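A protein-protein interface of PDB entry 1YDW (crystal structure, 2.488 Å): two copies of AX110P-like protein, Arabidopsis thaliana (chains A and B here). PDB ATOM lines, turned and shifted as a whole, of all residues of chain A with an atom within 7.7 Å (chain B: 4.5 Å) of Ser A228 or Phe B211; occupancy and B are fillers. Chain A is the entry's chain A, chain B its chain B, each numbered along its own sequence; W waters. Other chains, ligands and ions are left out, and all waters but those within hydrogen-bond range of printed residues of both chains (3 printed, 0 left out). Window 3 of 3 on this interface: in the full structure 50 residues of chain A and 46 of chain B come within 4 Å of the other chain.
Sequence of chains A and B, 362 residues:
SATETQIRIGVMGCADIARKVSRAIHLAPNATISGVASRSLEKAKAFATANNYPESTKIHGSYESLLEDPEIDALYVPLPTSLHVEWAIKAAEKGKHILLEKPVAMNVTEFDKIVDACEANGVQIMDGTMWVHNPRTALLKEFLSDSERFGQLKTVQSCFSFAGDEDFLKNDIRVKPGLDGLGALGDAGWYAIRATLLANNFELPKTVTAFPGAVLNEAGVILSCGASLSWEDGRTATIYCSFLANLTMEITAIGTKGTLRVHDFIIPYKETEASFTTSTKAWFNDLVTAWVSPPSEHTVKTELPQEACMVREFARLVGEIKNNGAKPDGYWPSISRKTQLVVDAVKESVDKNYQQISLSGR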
ATOM      1  N   THR A 155      -4.858 -29.485  23.370  1.00  0.00           N
ATOM      2  CA  THR A 155      -6.032 -28.665  23.604  1.00  0.00           C
ATOM      3  C   THR A 155      -5.651 -27.242  23.363  1.00  0.00           C
ATOM      4  O   THR A 155      -4.451 -26.880  23.417  1.00  0.00           O
ATOM      5  CB  THR A 155      -6.661 -28.843  25.021  1.00  0.00           C
ATOM      6  OG1 THR A 155      -8.017 -28.365  24.998  1.00  0.00           O
ATOM      7  CG2 THR A 155      -5.942 -28.088  26.000  1.00  0.00           C
ATOM      8  N   GLN A 157      -7.442 -23.346  24.208  1.00  0.00           N
ATOM      9  CA  GLN A 157      -8.482 -22.574  24.923  1.00  0.00           C
ATOM     10  C   GLN A 157      -8.414 -21.162  24.398  1.00  0.00           C
ATOM     11  O   GLN A 157      -7.323 -20.539  24.348  1.00  0.00           O
ATOM     12  CB  GLN A 157      -8.210 -22.481  26.426  1.00  0.00           C
ATOM     13  CG  GLN A 157      -8.686 -23.646  27.332  1.00  0.00           C
ATOM     14  CD  GLN A 157      -7.543 -24.526  27.927  1.00  0.00           C
ATOM     15  OE1 GLN A 157      -6.366 -24.178  27.885  1.00  0.00           O
ATOM     16  NE2 GLN A 157      -7.914 -25.655  28.481  1.00  0.00           N
ATOM     17  N   PRO A 205     -13.462 -29.547  13.989  1.00  0.00           N
ATOM     18  CA  PRO A 205     -13.608 -30.592  15.015  1.00  0.00           C
ATOM     19  C   PRO A 205     -14.643 -31.563  14.464  1.00  0.00           C
ATOM     20  O   PRO A 205     -15.064 -31.381  13.344  1.00  0.00           O
ATOM     21  CB  PRO A 205     -14.228 -29.829  16.192  1.00  0.00           C
ATOM     22  CG  PRO A 205     -14.899 -28.605  15.527  1.00  0.00           C
ATOM     23  CD  PRO A 205     -13.889 -28.231  14.496  1.00  0.00           C
ATOM     24  N   THR A 207     -17.430 -32.839  16.713  1.00  0.00           N
ATOM     25  CA  THR A 207     -18.649 -32.421  17.373  1.00  0.00           C
ATOM     26  C   THR A 207     -18.414 -31.100  18.089  1.00  0.00           C
ATOM     27  O   THR A 207     -17.269 -30.649  18.251  1.00  0.00           O
ATOM     28  CB  THR A 207     -19.181 -33.489  18.367  1.00  0.00           C
ATOM     29  OG1 THR A 207     -18.205 -33.718  19.381  1.00  0.00           O
ATOM     30  CG2 THR A 207     -19.443 -34.815  17.643  1.00  0.00           C
ATOM     31  N   VAL A 208     -19.513 -30.476  18.485  1.00  0.00           N
ATOM     32  CA  VAL A 208     -19.457 -29.199  19.120  1.00  0.00           C
ATOM     33  C   VAL A 208     -20.554 -29.325  20.086  1.00  0.00           C
ATOM     34  O   VAL A 208     -21.652 -29.824  19.709  1.00  0.00           O
ATOM     35  CB  VAL A 208     -19.852 -28.080  18.182  1.00  0.00           C
ATOM     36  CG1 VAL A 208     -20.196 -26.818  18.982  1.00  0.00           C
ATOM     37  CG2 VAL A 208     -18.768 -27.810  17.158  1.00  0.00           C
ATOM     38  N   THR A 209     -20.256 -28.900  21.335  1.00  0.00           N
ATOM     39  CA  THR A 209     -21.239 -28.887  22.435  1.00  0.00           C
ATOM     40  C   THR A 209     -21.113 -27.614  23.267  1.00  0.00           C
ATOM     41  O   THR A 209     -20.053 -27.324  23.825  1.00  0.00           O
ATOM     42  CB  THR A 209     -21.021 -30.079  23.357  1.00  0.00           C
ATOM     43  OG1 THR A 209     -20.620 -31.216  22.576  1.00  0.00           O
ATOM     44  CG2 THR A 209     -22.266 -30.390  24.177  1.00  0.00           C
ATOM     45  N   ALA A 210     -22.212 -26.873  23.367  1.00  0.00           N
ATOM     46  CA  ALA A 210     -22.249 -25.626  24.104  1.00  0.00           C
ATOM     47  C   ALA A 210     -22.235 -25.922  25.586  1.00  0.00           C
ATOM     48  O   ALA A 210     -22.745 -26.937  25.990  1.00  0.00           O
ATOM     49  CB  ALA A 210     -23.524 -24.884  23.737  1.00  0.00           C
ATOM     50  N   PHE A 211     -21.677 -25.021  26.397  1.00  0.00           N
ATOM     51  CA  PHE A 211     -21.762 -25.101  27.866  1.00  0.00           C
ATOM     52  C   PHE A 211     -23.132 -24.655  28.286  1.00  0.00           C
ATOM     53  O   PHE A 211     -23.575 -23.597  27.863  1.00  0.00           O
ATOM     54  CB  PHE A 211     -20.826 -24.098  28.570  1.00  0.00           C
ATOM     55  CG  PHE A 211     -19.419 -24.169  28.147  1.00  0.00           C
ATOM     56  CD1 PHE A 211     -18.861 -25.377  27.727  1.00  0.00           C
ATOM     57  CD2 PHE A 211     -18.626 -23.017  28.185  1.00  0.00           C
ATOM     58  CE1 PHE A 211     -17.520 -25.439  27.323  1.00  0.00           C
ATOM     59  CE2 PHE A 211     -17.281 -23.073  27.808  1.00  0.00           C
ATOM     60  CZ  PHE A 211     -16.729 -24.304  27.371  1.00  0.00           C
ATOM     61  N   GLY A 226     -20.318 -20.409  25.634  1.00  0.00           N
ATOM     62  CA  GLY A 226     -19.065 -21.142  25.387  1.00  0.00           C
ATOM     63  C   GLY A 226     -19.346 -22.558  24.863  1.00  0.00           C
ATOM     64  O   GLY A 226     -20.508 -22.972  24.705  1.00  0.00           O
ATOM     65  N   ALA A 227     -18.296 -23.334  24.605  1.00  0.00           N
ATOM     66  CA  ALA A 227     -18.493 -24.649  24.004  1.00  0.00           C
ATOM     67  C   ALA A 227     -17.202 -25.398  23.992  1.00  0.00           C
ATOM     68  O   ALA A 227     -16.143 -24.798  24.001  1.00  0.00           O
ATOM     69  CB  ALA A 227     -19.012 -24.507  22.517  1.00  0.00           C
ATOM     70  N   SER A 228     -17.275 -26.706  23.900  1.00  0.00           N
ATOM     71  CA  SER A 228     -16.081 -27.481  23.555  1.00  0.00           C
ATOM     72  C   SER A 228     -16.204 -28.137  22.195  1.00  0.00           C
ATOM     73  O   SER A 228     -17.287 -28.413  21.707  1.00  0.00           O
ATOM     74  CB  SER A 228     -15.703 -28.511  24.653  1.00  0.00           C
ATOM     75  OG  SER A 228     -16.804 -29.291  25.026  1.00  0.00           O
ATOM     76  N   LEU A 229     -15.064 -28.370  21.589  1.00  0.00           N
ATOM     77  CA  LEU A 229     -15.014 -29.026  20.304  1.00  0.00           C
ATOM     78  C   LEU A 229     -14.196 -30.293  20.515  1.00  0.00           C
ATOM     79  O   LEU A 229     -13.147 -30.241  21.144  1.00  0.00           O
ATOM     80  CB  LEU A 229     -14.315 -28.123  19.268  1.00  0.00           C
ATOM     81  CG  LEU A 229     -14.329 -26.598  19.319  1.00  0.00           C
ATOM     82  CD1 LEU A 229     -13.753 -26.034  18.045  1.00  0.00           C
ATOM     83  CD2 LEU A 229     -15.680 -26.039  19.536  1.00  0.00           C
ATOM     84  N   SER A 230     -14.678 -31.427  20.037  1.00  0.00           N
ATOM     85  CA  SER A 230     -13.878 -32.676  20.068  1.00  0.00           C
ATOM     86  C   SER A 230     -13.463 -33.171  18.701  1.00  0.00           C
ATOM     87  O   SER A 230     -14.323 -33.403  17.849  1.00  0.00           O
ATOM     88  CB  SER A 230     -14.624 -33.799  20.799  1.00  0.00           C
ATOM     89  OG  SER A 230     -16.028 -33.665  20.629  1.00  0.00           O
ATOM     90  N   TRP A 231     -12.159 -33.328  18.500  1.00  0.00           N
ATOM     91  CA  TRP A 231     -11.650 -34.071  17.342  1.00  0.00           C
ATOM     92  C   TRP A 231     -11.568 -35.627  17.534  1.00  0.00           C
ATOM     93  O   TRP A 231     -10.990 -36.334  16.682  1.00  0.00           O
ATOM     94  CB  TRP A 231     -10.292 -33.542  16.910  1.00  0.00           C
ATOM     95  CG  TRP A 231     -10.305 -32.192  16.383  1.00  0.00           C
ATOM     96  CD1 TRP A 231     -10.175 -31.807  15.075  1.00  0.00           C
ATOM     97  CD2 TRP A 231     -10.419 -30.992  17.142  1.00  0.00           C
ATOM     98  NE1 TRP A 231     -10.212 -30.429  14.974  1.00  0.00           N
ATOM     99  CE2 TRP A 231     -10.361 -29.911  16.234  1.00  0.00           C
ATOM    100  CE3 TRP A 231     -10.580 -30.722  18.503  1.00  0.00           C
ATOM    101  CZ2 TRP A 231     -10.450 -28.593  16.650  1.00  0.00           C
ATOM    102  CZ3 TRP A 231     -10.677 -29.409  18.910  1.00  0.00           C
ATOM    103  CH2 TRP A 231     -10.606 -28.360  17.988  1.00  0.00           C
ATOM    104  N   THR A 236      -8.999 -31.539  22.031  1.00  0.00           N
ATOM    105  CA  THR A 236     -10.244 -30.838  22.345  1.00  0.00           C
ATOM    106  C   THR A 236      -9.951 -29.351  22.373  1.00  0.00           C
ATOM    107  O   THR A 236      -8.784 -28.880  22.437  1.00  0.00           O
ATOM    108  CB  THR A 236     -10.849 -31.198  23.747  1.00  0.00           C
ATOM    109  OG1 THR A 236      -9.976 -30.721  24.778  1.00  0.00           O
ATOM    110  CG2 THR A 236     -11.180 -32.695  23.958  1.00  0.00           C
ATOM    111  N   ALA A 237     -11.016 -28.577  22.393  1.00  0.00           N
ATOM    112  CA  ALA A 237     -10.816 -27.153  22.566  1.00  0.00           C
ATOM    113  C   ALA A 237     -12.029 -26.591  23.272  1.00  0.00           C
ATOM    114  O   ALA A 237     -13.129 -27.223  23.309  1.00  0.00           O
ATOM    115  CB  ALA A 237     -10.562 -26.481  21.209  1.00  0.00           C
ATOM    116  N   THR A 238     -11.839 -25.421  23.850  1.00  0.00           N
ATOM    117  CA  THR A 238     -12.976 -24.697  24.445  1.00  0.00           C
ATOM    118  C   THR A 238     -12.949 -23.265  23.951  1.00  0.00           C
ATOM    119  O   THR A 238     -11.902 -22.725  23.600  1.00  0.00           O
ATOM    120  CB  THR A 238     -12.889 -24.685  25.943  1.00  0.00           C
ATOM    121  OG1 THR A 238     -11.628 -24.103  26.336  1.00  0.00           O
ATOM    122  CG2 THR A 238     -12.996 -26.119  26.501  1.00  0.00           C
ATOM    123  N   ILE A 239     -14.099 -22.637  23.854  1.00  0.00           N
ATOM    124  CA  ILE A 239     -14.081 -21.227  23.439  1.00  0.00           C
ATOM    125  C   ILE A 239     -15.063 -20.576  24.340  1.00  0.00           C
ATOM    126  O   ILE A 239     -15.957 -21.251  24.859  1.00  0.00           O
ATOM    127  CB  ILE A 239     -14.369 -20.995  21.890  1.00  0.00           C
ATOM    128  CG1 ILE A 239     -15.670 -21.653  21.432  1.00  0.00           C
ATOM    129  CG2 ILE A 239     -13.253 -21.532  21.038  1.00  0.00           C
ATOM    130  CD1 ILE A 239     -16.853 -20.592  21.361  1.00  0.00           C
ATOM    131  N   VAL A 342     -18.632 -23.534  12.482  1.00  0.00           N
ATOM    132  CA  VAL A 342     -18.499 -23.729  13.935  1.00  0.00           C
ATOM    133  C   VAL A 342     -19.446 -22.830  14.745  1.00  0.00           C
ATOM    134  O   VAL A 342     -20.105 -23.280  15.738  1.00  0.00           O
ATOM    135  CB  VAL A 342     -17.043 -23.552  14.391  1.00  0.00           C
ATOM    136  CG1 VAL A 342     -16.913 -23.762  15.940  1.00  0.00           C
ATOM    137  CG2 VAL A 342     -16.107 -24.547  13.608  1.00  0.00           C
ATOM    138  N   VAL A 346     -22.252 -24.382  17.334  1.00  0.00           N
ATOM    139  CA  VAL A 346     -22.494 -23.748  18.672  1.00  0.00           C
ATOM    140  C   VAL A 346     -23.906 -23.274  18.908  1.00  0.00           C
ATOM    141  O   VAL A 346     -24.544 -23.656  19.906  1.00  0.00           O
ATOM    142  CB  VAL A 346     -21.586 -22.563  18.975  1.00  0.00           C
ATOM    143  CG1 VAL A 346     -21.995 -21.938  20.317  1.00  0.00           C
ATOM    144  CG2 VAL A 346     -20.183 -23.012  19.040  1.00  0.00           C
ATOM    145  N   SER A 349     -26.477 -26.094  18.887  1.00  0.00           N
ATOM    146  CA  SER A 349     -26.341 -26.686  20.228  1.00  0.00           C
ATOM    147  C   SER A 349     -27.073 -25.939  21.321  1.00  0.00           C
ATOM    148  O   SER A 349     -27.809 -26.555  22.051  1.00  0.00           O
ATOM    149  CB  SER A 349     -24.881 -26.851  20.659  1.00  0.00           C
ATOM    150  OG  SER A 349     -24.819 -27.597  21.891  1.00  0.00           O
ATOM    151  N   GLN A 356     -25.065 -32.350  21.810  1.00  0.00           N
ATOM    152  CA  GLN A 356     -23.876 -32.417  20.977  1.00  0.00           C
ATOM    153  C   GLN A 356     -24.383 -32.306  19.537  1.00  0.00           C
ATOM    154  O   GLN A 356     -25.543 -32.675  19.252  1.00  0.00           O
ATOM    155  CB  GLN A 356     -23.210 -33.747  21.200  1.00  0.00           C
ATOM    156  CG  GLN A 356     -21.934 -33.963  20.448  1.00  0.00           C
ATOM    157  CD  GLN A 356     -21.075 -35.056  21.090  1.00  0.00           C
ATOM    158  OE1 GLN A 356     -20.009 -35.393  20.579  1.00  0.00           O
ATOM    159  NE2 GLN A 356     -21.536 -35.600  22.228  1.00  0.00           N
ATOM    160  N   ILE A 357     -23.552 -31.755  18.649  1.00  0.00           N
ATOM    161  CA  ILE A 357     -23.973 -31.461  17.286  1.00  0.00           C
ATOM    162  C   ILE A 357     -22.881 -32.005  16.467  1.00  0.00           C
ATOM    163  O   ILE A 357     -21.716 -31.632  16.652  1.00  0.00           O
ATOM    164  CB  ILE A 357     -24.059 -29.924  16.979  1.00  0.00           C
ATOM    165  CG1 ILE A 357     -25.140 -29.292  17.809  1.00  0.00           C
ATOM    166  CG2 ILE A 357     -24.346 -29.655  15.507  1.00  0.00           C
ATOM    167  CD1 ILE A 357     -26.405 -30.089  17.802  1.00  0.00           C
ATOM    168  N   THR B 209     -20.970 -30.782  33.861  1.00  0.00           N
ATOM    169  CA  THR B 209     -21.094 -31.593  32.648  1.00  0.00           C
ATOM    170  C   THR B 209     -19.728 -31.751  32.054  1.00  0.00           C
ATOM    171  O   THR B 209     -19.082 -30.757  31.754  1.00  0.00           O
ATOM    172  CB  THR B 209     -21.961 -30.863  31.573  1.00  0.00           C
ATOM    173  OG1 THR B 209     -23.088 -30.192  32.184  1.00  0.00           O
ATOM    174  CG2 THR B 209     -22.460 -31.875  30.491  1.00  0.00           C
ATOM    175  N   ALA B 210     -19.246 -32.963  31.876  1.00  0.00           N
ATOM    176  CA  ALA B 210     -17.875 -33.095  31.385  1.00  0.00           C
ATOM    177  C   ALA B 210     -17.823 -32.835  29.867  1.00  0.00           C
ATOM    178  O   ALA B 210     -18.819 -32.993  29.215  1.00  0.00           O
ATOM    179  CB  ALA B 210     -17.304 -34.482  31.731  1.00  0.00           C
ATOM    180  N   PHE B 211     -16.674 -32.435  29.334  1.00  0.00           N
ATOM    181  CA  PHE B 211     -16.452 -32.370  27.883  1.00  0.00           C
ATOM    182  C   PHE B 211     -16.325 -33.720  27.235  1.00  0.00           C
ATOM    183  O   PHE B 211     -15.549 -34.554  27.694  1.00  0.00           O
ATOM    184  CB  PHE B 211     -15.098 -31.713  27.570  1.00  0.00           C
ATOM    185  CG  PHE B 211     -14.881 -30.406  28.235  1.00  0.00           C
ATOM    186  CD1 PHE B 211     -15.956 -29.624  28.677  1.00  0.00           C
ATOM    187  CD2 PHE B 211     -13.611 -29.893  28.335  1.00  0.00           C
ATOM    188  CE1 PHE B 211     -15.730 -28.392  29.255  1.00  0.00           C
ATOM    189  CE2 PHE B 211     -13.403 -28.599  28.899  1.00  0.00           C
ATOM    190  CZ  PHE B 211     -14.463 -27.883  29.342  1.00  0.00           C
ATOM    191  N   PRO B 212     -17.022 -33.945  26.118  1.00  0.00           N
ATOM    192  CA  PRO B 212     -16.658 -35.143  25.326  1.00  0.00           C
ATOM    193  C   PRO B 212     -15.163 -35.206  25.090  1.00  0.00           C
ATOM    194  O   PRO B 212     -14.498 -34.186  25.170  1.00  0.00           O
ATOM    195  CB  PRO B 212     -17.380 -34.906  24.037  1.00  0.00           C
ATOM    196  CG  PRO B 212     -18.686 -34.165  24.489  1.00  0.00           C
ATOM    197  CD  PRO B 212     -18.188 -33.218  25.560  1.00  0.00           C
ATOM    198  N   GLY B 213     -14.629 -36.394  24.831  1.00  0.00           N
ATOM    199  CA  GLY B 213     -13.228 -36.567  24.508  1.00  0.00           C
ATOM    200  C   GLY B 213     -12.342 -36.757  25.716  1.00  0.00           C
ATOM    201  O   GLY B 213     -11.137 -36.502  25.645  1.00  0.00           O
ATOM    202  N   ALA B 214     -12.881 -37.210  26.847  1.00  0.00           N
ATOM    203  CA  ALA B 214     -11.958 -37.558  27.956  1.00  0.00           C
ATOM    204  C   ALA B 214     -11.034 -38.764  27.577  1.00  0.00           C
ATOM    205  O   ALA B 214     -11.513 -39.768  27.089  1.00  0.00           O
ATOM    206  CB  ALA B 214     -12.747 -37.864  29.183  1.00  0.00           C
ATOM    207  N   GLY B 226     -12.210 -32.691  31.049  1.00  0.00           N
ATOM    208  CA  GLY B 226     -12.637 -31.322  31.289  1.00  0.00           C
ATOM    209  C   GLY B 226     -14.101 -31.211  31.596  1.00  0.00           C
ATOM    210  O   GLY B 226     -14.840 -32.174  31.483  1.00  0.00           O
ATOM    211  N   ALA B 227     -14.547 -30.006  31.925  1.00  0.00           N
ATOM    212  CA  ALA B 227     -15.916 -29.846  32.367  1.00  0.00           C
ATOM    213  C   ALA B 227     -16.316 -28.405  32.320  1.00  0.00           C
ATOM    214  O   ALA B 227     -15.480 -27.540  32.541  1.00  0.00           O
ATOM    215  CB  ALA B 227     -16.051 -30.334  33.879  1.00  0.00           C
ATOM    216  N   SER B 228     -17.602 -28.151  32.197  1.00  0.00           N
ATOM    217  CA  SER B 228     -18.119 -26.816  32.528  1.00  0.00           C
ATOM    218  C   SER B 228     -18.967 -26.980  33.731  1.00  0.00           C
ATOM    219  O   SER B 228     -19.575 -28.052  33.867  1.00  0.00           O
ATOM    220  CB  SER B 228     -18.921 -26.166  31.383  1.00  0.00           C
ATOM    221  OG  SER B 228     -19.813 -27.070  30.758  1.00  0.00           O
ATOM    222  N   THR B 238     -14.934 -23.312  33.626  1.00  0.00           N
ATOM    223  CA  THR B 238     -14.414 -24.492  32.996  1.00  0.00           C
ATOM    224  C   THR B 238     -13.179 -24.973  33.717  1.00  0.00           C
ATOM    225  O   THR B 238     -12.315 -24.180  34.142  1.00  0.00           O
ATOM    226  CB  THR B 238     -14.091 -24.321  31.505  1.00  0.00           C
ATOM    227  OG1 THR B 238     -13.256 -23.170  31.314  1.00  0.00           O
ATOM    228  CG2 THR B 238     -15.314 -24.166  30.688  1.00  0.00           C
ATOM    229  N   ILE B 239     -13.086 -26.292  33.834  1.00  0.00           N
ATOM    230  CA  ILE B 239     -11.835 -26.896  34.285  1.00  0.00           C
ATOM    231  C   ILE B 239     -11.222 -27.746  33.202  1.00  0.00           C
ATOM    232  O   ILE B 239     -11.914 -28.304  32.340  1.00  0.00           O
ATOM    233  CB  ILE B 239     -11.999 -27.662  35.650  1.00  0.00           C
ATOM    234  CG1 ILE B 239     -13.094 -28.697  35.589  1.00  0.00           C
ATOM    235  CG2 ILE B 239     -12.314 -26.708  36.722  1.00  0.00           C
ATOM    236  CD1 ILE B 239     -12.520 -30.114  35.447  1.00  0.00           C
ATOM    237  N   TYR B 354     -21.195 -38.221  29.344  1.00  0.00           N
ATOM    238  CA  TYR B 354     -21.165 -36.749  29.251  1.00  0.00           C
ATOM    239  C   TYR B 354     -22.525 -36.114  29.515  1.00  0.00           C
ATOM    240  O   TYR B 354     -22.851 -35.100  28.953  1.00  0.00           O
ATOM    241  CB  TYR B 354     -20.518 -36.297  27.948  1.00  0.00           C
ATOM    242  CG  TYR B 354     -19.158 -36.953  27.747  1.00  0.00           C
ATOM    243  CD1 TYR B 354     -18.964 -38.020  26.828  1.00  0.00           C
ATOM    244  CD2 TYR B 354     -18.059 -36.539  28.506  1.00  0.00           C
ATOM    245  CE1 TYR B 354     -17.689 -38.625  26.662  1.00  0.00           C
ATOM    246  CE2 TYR B 354     -16.804 -37.138  28.347  1.00  0.00           C
ATOM    247  CZ  TYR B 354     -16.625 -38.179  27.432  1.00  0.00           C
ATOM    248  OH  TYR B 354     -15.341 -38.697  27.321  1.00  0.00           O
HETATM  249  O   HOH W   1     -16.116 -32.145  23.987  1.00  0.00           O
HETATM  250  O   HOH W   2     -14.720 -36.589  21.635  1.00  0.00           O
HETATM  251  O   HOH W   3     -12.190 -24.107  28.918  1.00  0.00           O
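OG1 of Thr A207 is in hydrogen-bond range of OG of Ser A230, at 2.5 Å.
O of Thr A209 lies within hydrogen-bond range of N of Ser A228, 2.8 Å away.
OG1 of Thr A155 is in hydrogen-bond range of O of Thr A236 (2.7 Å).
The side-chain hydroxyl of Thr A207 sits at hydrogen-bond distance from the side-chain amide oxygen of Gln A356, 2.7 Å away.
N of Phe A211 sits at hydrogen-bond distance from O of Gly A226 (2.9 Å).
The backbone carbonyl oxygen (O) of Thr B209 lies within hydrogen-bond range of the backbone NH (N) of Ser B228 (3.0 Å).
Among the printed residues, pairs that only touch across the chains: Thr A238 with Phe B211, Phe A211 with Ser B228, Phe A211 with Thr B238, Ser A228 with Phe B211, Thr A236 with Pro B212, Ser A230 with Pro B212, Gln A356 with Pro B212 and Phe A211 with Phe B211.
Of chain B, only Phe B211 comes within 4 Å of Ser A228.
Of the printed residues of chain B, Ser A230 touches Pro B212.
Printed residues of chain B within 4 Å of Thr A238: Phe B211.
Phe B211 touches just these residues of chain A: Phe A211 (3.96 Å), Ser A228 (3.8 Å) and Thr A238 (3.5 Å).
Of the printed residues of chain A, Ser B228 touches Phe A211.
The nearest residue of chain B that does not touch Ser A228 is Pro B212 (4.2 Å).
The nearest residue of chain A that does not touch Phe B211 is Thr A236 (5.2 Å).
Of the 23 printed residues of chain A, 6 touch a printed residue of chain B.
Printed residues of chain B that touch a printed residue of chain A: Phe B211, Pro B212, Ser B228 and Thr B238.
Hydrophobic or aromatic side chains of chain B that line the printed part of chain A: Phe B211 and Pro B212.
Among the printed residues, no Asp or Glu carboxylate lies within 4 Å of a Lys or Arg side-chain nitrogen of the other chain.
Phe B211 touches its own counterpart, Phe A211.
Phe A211 touches Ser B228, and with the chains exchanged Ser A228 touches Phe B211.
Phe A211 touches Thr B238, and with the chains exchanged Thr A238 touches Phe B211.
Positions printed for both chains: 209, 210, 211, 226, 227, 228, 238 and 239.
Water W3 bridges the side-chain hydroxyl of Thr A238 (2.6 Å) and the side-chain hydroxyl of Thr B238 (2.8 Å).
Water W1 lies within hydrogen-bond range of O of Pro B212 (2.9 Å) and OG of Ser A228 (3.1 Å).
Water W2 bridges N of Gly B213 (3.2 Å) and OG of Ser A230 (3.4 Å).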
